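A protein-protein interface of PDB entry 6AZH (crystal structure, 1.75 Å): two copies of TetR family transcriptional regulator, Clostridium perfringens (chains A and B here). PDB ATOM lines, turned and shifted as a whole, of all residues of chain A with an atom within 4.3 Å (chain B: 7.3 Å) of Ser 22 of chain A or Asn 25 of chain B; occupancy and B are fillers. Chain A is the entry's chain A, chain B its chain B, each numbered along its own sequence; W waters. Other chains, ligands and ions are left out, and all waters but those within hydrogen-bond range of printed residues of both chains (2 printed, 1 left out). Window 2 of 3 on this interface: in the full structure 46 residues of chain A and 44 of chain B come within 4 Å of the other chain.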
ATOM      1  N   VAL A  18     -19.063 -22.054   2.936  1.00  0.00           N
ATOM      2  CA  VAL A  18     -20.140 -22.697   2.183  1.00  0.00           C
ATOM      3  C   VAL A  18     -19.688 -22.989   0.757  1.00  0.00           C
ATOM      4  O   VAL A  18     -19.793 -24.124   0.272  1.00  0.00           O
ATOM      5  CB  VAL A  18     -21.409 -21.827   2.201  1.00  0.00           C
ATOM      6  CG1 VAL A  18     -22.462 -22.440   1.306  1.00  0.00           C
ATOM      7  CG2 VAL A  18     -21.950 -21.697   3.636  1.00  0.00           C
ATOM      8  N   PHE A  19     -19.175 -21.967   0.066  1.00  0.00           N
ATOM      9  CA  PHE A  19     -18.678 -22.160  -1.295  1.00  0.00           C
ATOM     10  C   PHE A  19     -17.567 -23.215  -1.341  1.00  0.00           C
ATOM     11  O   PHE A  19     -17.521 -24.029  -2.266  1.00  0.00           O
ATOM     12  CB  PHE A  19     -18.172 -20.831  -1.866  1.00  0.00           C
ATOM     13  CG  PHE A  19     -19.259 -19.872  -2.272  1.00  0.00           C
ATOM     14  CD1 PHE A  19     -20.293 -20.283  -3.106  1.00  0.00           C
ATOM     15  CD2 PHE A  19     -19.226 -18.545  -1.846  1.00  0.00           C
ATOM     16  CE1 PHE A  19     -21.285 -19.391  -3.498  1.00  0.00           C
ATOM     17  CE2 PHE A  19     -20.210 -17.641  -2.231  1.00  0.00           C
ATOM     18  CZ  PHE A  19     -21.249 -18.066  -3.060  1.00  0.00           C
ATOM     19  N   ALA A  20     -16.660 -23.216  -0.360  1.00  0.00           N
ATOM     20  CA  ALA A  20     -15.571 -24.194  -0.393  1.00  0.00           C
ATOM     21  C   ALA A  20     -16.071 -25.609  -0.133  1.00  0.00           C
ATOM     22  O   ALA A  20     -15.517 -26.570  -0.674  1.00  0.00           O
ATOM     23  CB  ALA A  20     -14.485 -23.837   0.623  1.00  0.00           C
ATOM     24  N   THR A  21     -17.115 -25.752   0.675  1.00  0.00           N
ATOM     25  CA  THR A  21     -17.633 -27.071   1.016  1.00  0.00           C
ATOM     26  C   THR A  21     -18.497 -27.638  -0.108  1.00  0.00           C
ATOM     27  O   THR A  21     -18.322 -28.789  -0.522  1.00  0.00           O
ATOM     28  CB  THR A  21     -18.434 -26.969   2.318  1.00  0.00           C
ATOM     29  OG1 THR A  21     -17.536 -26.674   3.396  1.00  0.00           O
ATOM     30  CG2 THR A  21     -19.181 -28.273   2.604  1.00  0.00           C
ATOM     31  N   SER A  22     -19.432 -26.835  -0.613  1.00  0.00           N
ATOM     32  CA  SER A  22     -20.485 -27.310  -1.495  1.00  0.00           C
ATOM     33  C   SER A  22     -20.300 -26.912  -2.946  1.00  0.00           C
ATOM     34  O   SER A  22     -21.048 -27.401  -3.796  1.00  0.00           O
ATOM     35  CB  SER A  22     -21.847 -26.782  -1.015  1.00  0.00           C
ATOM     36  OG  SER A  22     -22.033 -27.087   0.349  1.00  0.00           O
ATOM     37  N   GLY A  23     -19.341 -26.041  -3.255  1.00  0.00           N
ATOM     38  CA  GLY A  23     -19.233 -25.507  -4.597  1.00  0.00           C
ATOM     39  C   GLY A  23     -20.294 -24.462  -4.870  1.00  0.00           C
ATOM     40  O   GLY A  23     -21.223 -24.274  -4.071  1.00  0.00           O
ATOM     41  N   ASN A  25     -22.807 -24.077  -7.277  1.00  0.00           N
ATOM     42  CA  ASN A  25     -24.203 -24.432  -7.547  1.00  0.00           C
ATOM     43  C   ASN A  25     -24.898 -24.977  -6.304  1.00  0.00           C
ATOM     44  O   ASN A  25     -26.100 -24.745  -6.098  1.00  0.00           O
ATOM     45  CB  ASN A  25     -24.284 -25.454  -8.684  1.00  0.00           C
ATOM     46  CG  ASN A  25     -24.032 -24.836 -10.049  1.00  0.00           C
ATOM     47  OD1 ASN A  25     -24.041 -23.615 -10.205  1.00  0.00           O
ATOM     48  ND2 ASN A  25     -23.791 -25.682 -11.043  1.00  0.00           N
ATOM     49  N   GLY A  26     -24.170 -25.732  -5.479  1.00  0.00           N
ATOM     50  CA  GLY A  26     -24.722 -26.302  -4.267  1.00  0.00           C
ATOM     51  C   GLY A  26     -24.853 -25.346  -3.103  1.00  0.00           C
ATOM     52  O   GLY A  26     -25.550 -25.665  -2.138  1.00  0.00           O
ATOM     53  N   SER A  27     -24.195 -24.191  -3.163  1.00  0.00           N
ATOM     54  CA  SER A  27     -24.338 -23.175  -2.132  1.00  0.00           C
ATOM     55  C   SER A  27     -25.614 -22.381  -2.361  1.00  0.00           C
ATOM     56  O   SER A  27     -26.101 -22.269  -3.489  1.00  0.00           O
ATOM     57  CB  SER A  27     -23.137 -22.241  -2.137  1.00  0.00           C
ATOM     58  OG  SER A  27     -21.932 -22.988  -1.999  1.00  0.00           O
ATOM     59  N   PHE B  19     -21.804 -32.125 -17.137  1.00  0.00           N
ATOM     60  CA  PHE B  19     -21.146 -31.848 -15.858  1.00  0.00           C
ATOM     61  C   PHE B  19     -20.294 -30.587 -15.947  1.00  0.00           C
ATOM     62  O   PHE B  19     -20.228 -29.804 -14.993  1.00  0.00           O
ATOM     63  CB  PHE B  19     -20.283 -33.036 -15.417  1.00  0.00           C
ATOM     64  CG  PHE B  19     -21.073 -34.250 -14.992  1.00  0.00           C
ATOM     65  CD1 PHE B  19     -22.267 -34.110 -14.303  1.00  0.00           C
ATOM     66  CD2 PHE B  19     -20.618 -35.527 -15.287  1.00  0.00           C
ATOM     67  CE1 PHE B  19     -23.000 -35.231 -13.913  1.00  0.00           C
ATOM     68  CE2 PHE B  19     -21.336 -36.650 -14.906  1.00  0.00           C
ATOM     69  CZ  PHE B  19     -22.534 -36.502 -14.216  1.00  0.00           C
ATOM     70  N   SER B  22     -23.447 -27.633 -16.634  1.00  0.00           N
ATOM     71  CA  SER B  22     -24.473 -27.487 -15.611  1.00  0.00           C
ATOM     72  C   SER B  22     -23.977 -27.845 -14.219  1.00  0.00           C
ATOM     73  O   SER B  22     -24.742 -27.739 -13.259  1.00  0.00           O
ATOM     74  CB  SER B  22     -25.691 -28.350 -15.953  1.00  0.00           C
ATOM     75  OG  SER B  22     -26.112 -28.111 -17.280  1.00  0.00           O
ATOM     76  N   GLY B  23     -22.725 -28.270 -14.091  1.00  0.00           N
ATOM     77  CA  GLY B  23     -22.213 -28.753 -12.829  1.00  0.00           C
ATOM     78  C   GLY B  23     -22.713 -30.153 -12.535  1.00  0.00           C
ATOM     79  O   GLY B  23     -23.558 -30.721 -13.235  1.00  0.00           O
ATOM     80  N   TYR B  24     -22.148 -30.742 -11.485  1.00  0.00           N
ATOM     81  CA  TYR B  24     -22.731 -31.967 -10.961  1.00  0.00           C
ATOM     82  C   TYR B  24     -23.998 -31.642 -10.188  1.00  0.00           C
ATOM     83  O   TYR B  24     -25.091 -32.124 -10.514  1.00  0.00           O
ATOM     84  CB  TYR B  24     -21.734 -32.704 -10.067  1.00  0.00           C
ATOM     85  CG  TYR B  24     -22.339 -33.965  -9.503  1.00  0.00           C
ATOM     86  CD1 TYR B  24     -22.355 -35.143 -10.248  1.00  0.00           C
ATOM     87  CD2 TYR B  24     -22.936 -33.970  -8.251  1.00  0.00           C
ATOM     88  CE1 TYR B  24     -22.928 -36.299  -9.742  1.00  0.00           C
ATOM     89  CE2 TYR B  24     -23.513 -35.113  -7.738  1.00  0.00           C
ATOM     90  CZ  TYR B  24     -23.509 -36.273  -8.484  1.00  0.00           C
ATOM     91  OH  TYR B  24     -24.082 -37.405  -7.960  1.00  0.00           O
ATOM     92  N   ASN B  25     -23.864 -30.827  -9.146  1.00  0.00           N
ATOM     93  CA  ASN B  25     -25.023 -30.156  -8.588  1.00  0.00           C
ATOM     94  C   ASN B  25     -25.543 -29.175  -9.625  1.00  0.00           C
ATOM     95  O   ASN B  25     -24.786 -28.348 -10.140  1.00  0.00           O
ATOM     96  CB  ASN B  25     -24.643 -29.443  -7.293  1.00  0.00           C
ATOM     97  CG  ASN B  25     -24.085 -30.395  -6.262  1.00  0.00           C
ATOM     98  OD1 ASN B  25     -24.575 -31.521  -6.114  1.00  0.00           O
ATOM     99  ND2 ASN B  25     -23.050 -29.960  -5.545  1.00  0.00           N
ATOM    100  N   GLY B  26     -26.824 -29.289  -9.966  1.00  0.00           N
ATOM    101  CA  GLY B  26     -27.414 -28.494 -11.021  1.00  0.00           C
ATOM    102  C   GLY B  26     -27.691 -29.260 -12.300  1.00  0.00           C
ATOM    103  O   GLY B  26     -28.446 -28.772 -13.149  1.00  0.00           O
ATOM    104  N   SER B  27     -27.090 -30.425 -12.480  1.00  0.00           N
ATOM    105  CA  SER B  27     -27.439 -31.283 -13.599  1.00  0.00           C
ATOM    106  C   SER B  27     -28.379 -32.382 -13.128  1.00  0.00           C
ATOM    107  O   SER B  27     -28.514 -32.650 -11.931  1.00  0.00           O
ATOM    108  CB  SER B  27     -26.199 -31.905 -14.234  1.00  0.00           C
ATOM    109  OG  SER B  27     -25.623 -32.878 -13.379  1.00  0.00           O
ATOM    110  N   THR B  28     -29.025 -33.022 -14.095  1.00  0.00           N
ATOM    111  CA  THR B  28     -29.939 -34.120 -13.832  1.00  0.00           C
ATOM    112  C   THR B  28     -29.604 -35.282 -14.746  1.00  0.00           C
ATOM    113  O   THR B  28     -28.973 -35.117 -15.794  1.00  0.00           O
ATOM    114  CB  THR B  28     -31.401 -33.720 -14.069  1.00  0.00           C
ATOM    115  OG1 THR B  28     -31.576 -33.397 -15.459  1.00  0.00           O
ATOM    116  CG2 THR B  28     -31.783 -32.528 -13.202  1.00  0.00           C
ATOM    117  N   LYS B  50     -27.229 -40.431 -11.176  1.00  0.00           N
ATOM    118  CA  LYS B  50     -26.285 -39.430 -11.653  1.00  0.00           C
ATOM    119  C   LYS B  50     -24.912 -39.647 -11.028  1.00  0.00           C
ATOM    120  O   LYS B  50     -23.882 -39.447 -11.684  1.00  0.00           O
ATOM    121  CB  LYS B  50     -26.815 -38.030 -11.341  1.00  0.00           C
ATOM    122  CG  LYS B  50     -26.003 -36.899 -11.983  1.00  0.00           C
ATOM    123  CD  LYS B  50     -26.629 -35.541 -11.685  1.00  0.00           C
ATOM    124  CE  LYS B  50     -26.399 -35.099 -10.240  1.00  0.00           C
ATOM    125  NZ  LYS B  50     -27.156 -33.831  -9.970  1.00  0.00           N
ATOM    126  N   GLN B 107     -14.324 -30.001 -10.391  1.00  0.00           N
ATOM    127  CA  GLN B 107     -14.912 -30.885  -9.396  1.00  0.00           C
ATOM    128  C   GLN B 107     -13.936 -31.303  -8.303  1.00  0.00           C
ATOM    129  O   GLN B 107     -14.333 -32.020  -7.380  1.00  0.00           O
ATOM    130  CB  GLN B 107     -15.470 -32.128 -10.099  1.00  0.00           C
ATOM    131  CG  GLN B 107     -16.657 -31.813 -10.993  1.00  0.00           C
ATOM    132  CD  GLN B 107     -17.847 -31.312 -10.178  1.00  0.00           C
ATOM    133  OE1 GLN B 107     -18.136 -31.838  -9.118  1.00  0.00           O
ATOM    134  NE2 GLN B 107     -18.498 -30.269 -10.652  1.00  0.00           N
ATOM    135  N   GLY B 110     -14.135 -29.697  -3.648  1.00  0.00           N
ATOM    136  CA  GLY B 110     -15.174 -29.678  -2.638  1.00  0.00           C
ATOM    137  C   GLY B 110     -15.081 -30.849  -1.673  1.00  0.00           C
ATOM    138  O   GLY B 110     -14.156 -31.666  -1.712  1.00  0.00           O
ATOM    139  N   LYS B 111     -16.079 -30.931  -0.790  1.00  0.00           N
ATOM    140  CA  LYS B 111     -16.055 -31.884   0.316  1.00  0.00           C
ATOM    141  C   LYS B 111     -17.089 -32.997   0.187  1.00  0.00           C
ATOM    142  O   LYS B 111     -17.303 -33.744   1.146  1.00  0.00           O
ATOM    143  CB  LYS B 111     -16.242 -31.152   1.648  1.00  0.00           C
ATOM    144  CG  LYS B 111     -15.040 -30.315   2.054  1.00  0.00           C
ATOM    145  CD  LYS B 111     -15.407 -29.305   3.141  1.00  0.00           C
ATOM    146  CE  LYS B 111     -14.777 -29.653   4.482  1.00  0.00           C
ATOM    147  NZ  LYS B 111     -15.152 -28.658   5.538  1.00  0.00           N
ATOM    148  N   GLU B 112     -17.728 -33.139  -0.964  1.00  0.00           N
ATOM    149  CA  GLU B 112     -18.678 -34.224  -1.130  1.00  0.00           C
ATOM    150  C   GLU B 112     -17.929 -35.525  -1.428  1.00  0.00           C
ATOM    151  O   GLU B 112     -16.773 -35.513  -1.857  1.00  0.00           O
ATOM    152  CB  GLU B 112     -19.693 -33.852  -2.214  1.00  0.00           C
ATOM    153  CG  GLU B 112     -20.327 -32.474  -1.899  1.00  0.00           C
ATOM    154  CD  GLU B 112     -21.447 -32.052  -2.842  1.00  0.00           C
ATOM    155  OE1 GLU B 112     -21.606 -32.681  -3.912  1.00  0.00           O
ATOM    156  OE2 GLU B 112     -22.163 -31.073  -2.504  1.00  0.00           O
ATOM    157  N   ARG B 114     -18.166 -37.947  -3.601  1.00  0.00           N
ATOM    158  CA  ARG B 114     -17.714 -38.126  -4.978  1.00  0.00           C
ATOM    159  C   ARG B 114     -16.411 -37.370  -5.232  1.00  0.00           C
ATOM    160  O   ARG B 114     -15.612 -37.768  -6.087  1.00  0.00           O
ATOM    161  CB  ARG B 114     -18.800 -37.655  -5.955  1.00  0.00           C
ATOM    162  CG  ARG B 114     -18.620 -36.203  -6.385  1.00  0.00           C
ATOM    163  CD  ARG B 114     -19.428 -35.757  -7.600  1.00  0.00           C
ATOM    164  NE  ARG B 114     -19.464 -34.293  -7.676  1.00  0.00           N
ATOM    165  CZ  ARG B 114     -20.009 -33.495  -6.761  1.00  0.00           C
ATOM    166  NH1 ARG B 114     -20.625 -34.007  -5.700  1.00  0.00           N
ATOM    167  NH2 ARG B 114     -19.969 -32.178  -6.917  1.00  0.00           N
ATOM    168  N   GLN B 115     -16.189 -36.279  -4.502  1.00  0.00           N
ATOM    169  CA  GLN B 115     -14.993 -35.472  -4.709  1.00  0.00           C
ATOM    170  C   GLN B 115     -13.795 -36.054  -3.964  1.00  0.00           C
ATOM    171  O   GLN B 115     -12.675 -36.029  -4.485  1.00  0.00           O
ATOM    172  CB  GLN B 115     -15.283 -34.024  -4.299  1.00  0.00           C
ATOM    173  CG  GLN B 115     -16.419 -33.405  -5.126  1.00  0.00           C
ATOM    174  CD  GLN B 115     -16.768 -31.972  -4.714  1.00  0.00           C
ATOM    175  OE1 GLN B 115     -17.424 -31.750  -3.697  1.00  0.00           O
ATOM    176  NE2 GLN B 115     -16.325 -30.995  -5.510  1.00  0.00           N
HETATM  177  O   HOH W   1     -21.942 -27.315  -6.167  1.00  0.00           O
HETATM  178  O   HOH W   2     -22.285 -29.932   0.394  1.00  0.00           O
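The backbone carbonyl oxygen (O) of Gly 23 of chain B lies within hydrogen-bond range of the side-chain hydroxyl (OG) of Ser 27 of chain B, at 3.0 Å. ND2 of Asn 25 of chain B sits at hydrogen-bond distance from OE2 of Glu 112 of chain B, 3.4 Å away. The side-chain amide nitrogen (NE2) of Gln 115 of chain B lies close to the backbone NH (N) of Gly 110 of chain B (3.2 Å). The side-chain amide oxygen of Gln 115 of chain B sits at hydrogen-bond distance from the backbone NH of Lys 111 of chain B (3.3 Å).
Among the printed residues, pairs that only touch across the chains: Ser 22 of chain A with Asn 25 of chain B (3.7 Å), Ala 20 of chain A with Gly 110 of chain B (3.7 Å), Asn 25 of chain A with Gly 23 of chain B (3.9 Å) and Thr 21 of chain A with Gly 110 of chain B (3.9 Å).
O of Thr 21 of chain A sits at hydrogen-bond distance from N of Lys 111 of chain B (3.1 Å). ND2 of Asn 25 of chain A sits at hydrogen-bond distance from O of Ser 22 of chain B (3.2 Å). The side-chain amide nitrogen (ND2) of Asn 25 of chain A sits at hydrogen-bond distance from the backbone carbonyl oxygen (O) of Asn 25 of chain B (3.0 Å).
Water W1 lies within hydrogen-bond range of the backbone carbonyl oxygen (O) of Ser 22 of chain A (2.5 Å), the backbone NH (N) of Gly 26 of chain A (2.8 Å) and the side-chain amide nitrogen (ND2) of Asn 25 of chain B (2.9 Å). Water W2 bridges the side-chain hydroxyl (OG) of Ser 22 of chain A (2.9 Å) and the side-chain carboxylate (OE2) of Glu 112 of chain B (3.1 Å).
Phe 19 of chain A touches none of the printed residues of chain B. Of the printed residues of chain B, Ala 20 of chain A touches Gly 110. No residue of chain B comes within 4 Å of Gly 23 of chain A. Of the printed residues of chain B, Asn 25 of chain A touches Ser 22, Gly 23 and Asn 25. Printed residues of chain A within 4 Å of Gly 23 of chain B: Asn 25. Asn 25 of chain B touches just these residues of chain A: Ser 22 (3.7 Å) and Asn 25 (3.0 Å). Of the printed residues of chain A, Gly 110 of chain B touches Ala 20 and Thr 21. Printed residues of chain A within 4 Å of Lys 111 of chain B: Thr 21 (3.1 Å). The nearest residue of chain A that does not touch Asn 25 of chain B is Gly 26 of chain A (4.2 Å). The nearest printed residue of chain A that does not touch Ser 22 of chain B is Gly 26 of chain A (8.1 Å).
Among the printed residues, no Asp or Glu carboxylate lies within 4 Å of a Lys or Arg side-chain nitrogen of the other chain.
Ser 22 of chain A touches Asn 25 of chain B, and with the chains exchanged Asn 25 of chain A touches Ser 22 of chain B. Asn 25 of chain A touches Gly 23 of chain B, but with the chains exchanged Gly 23 of chain A does not touch Asn 25 of chain B (5.9 Å). Asn 25 of chain A touches its own counterpart, Asn 25 of chain B. Positions printed for both chains: 19, 22, 23, 25, 26 and 27.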
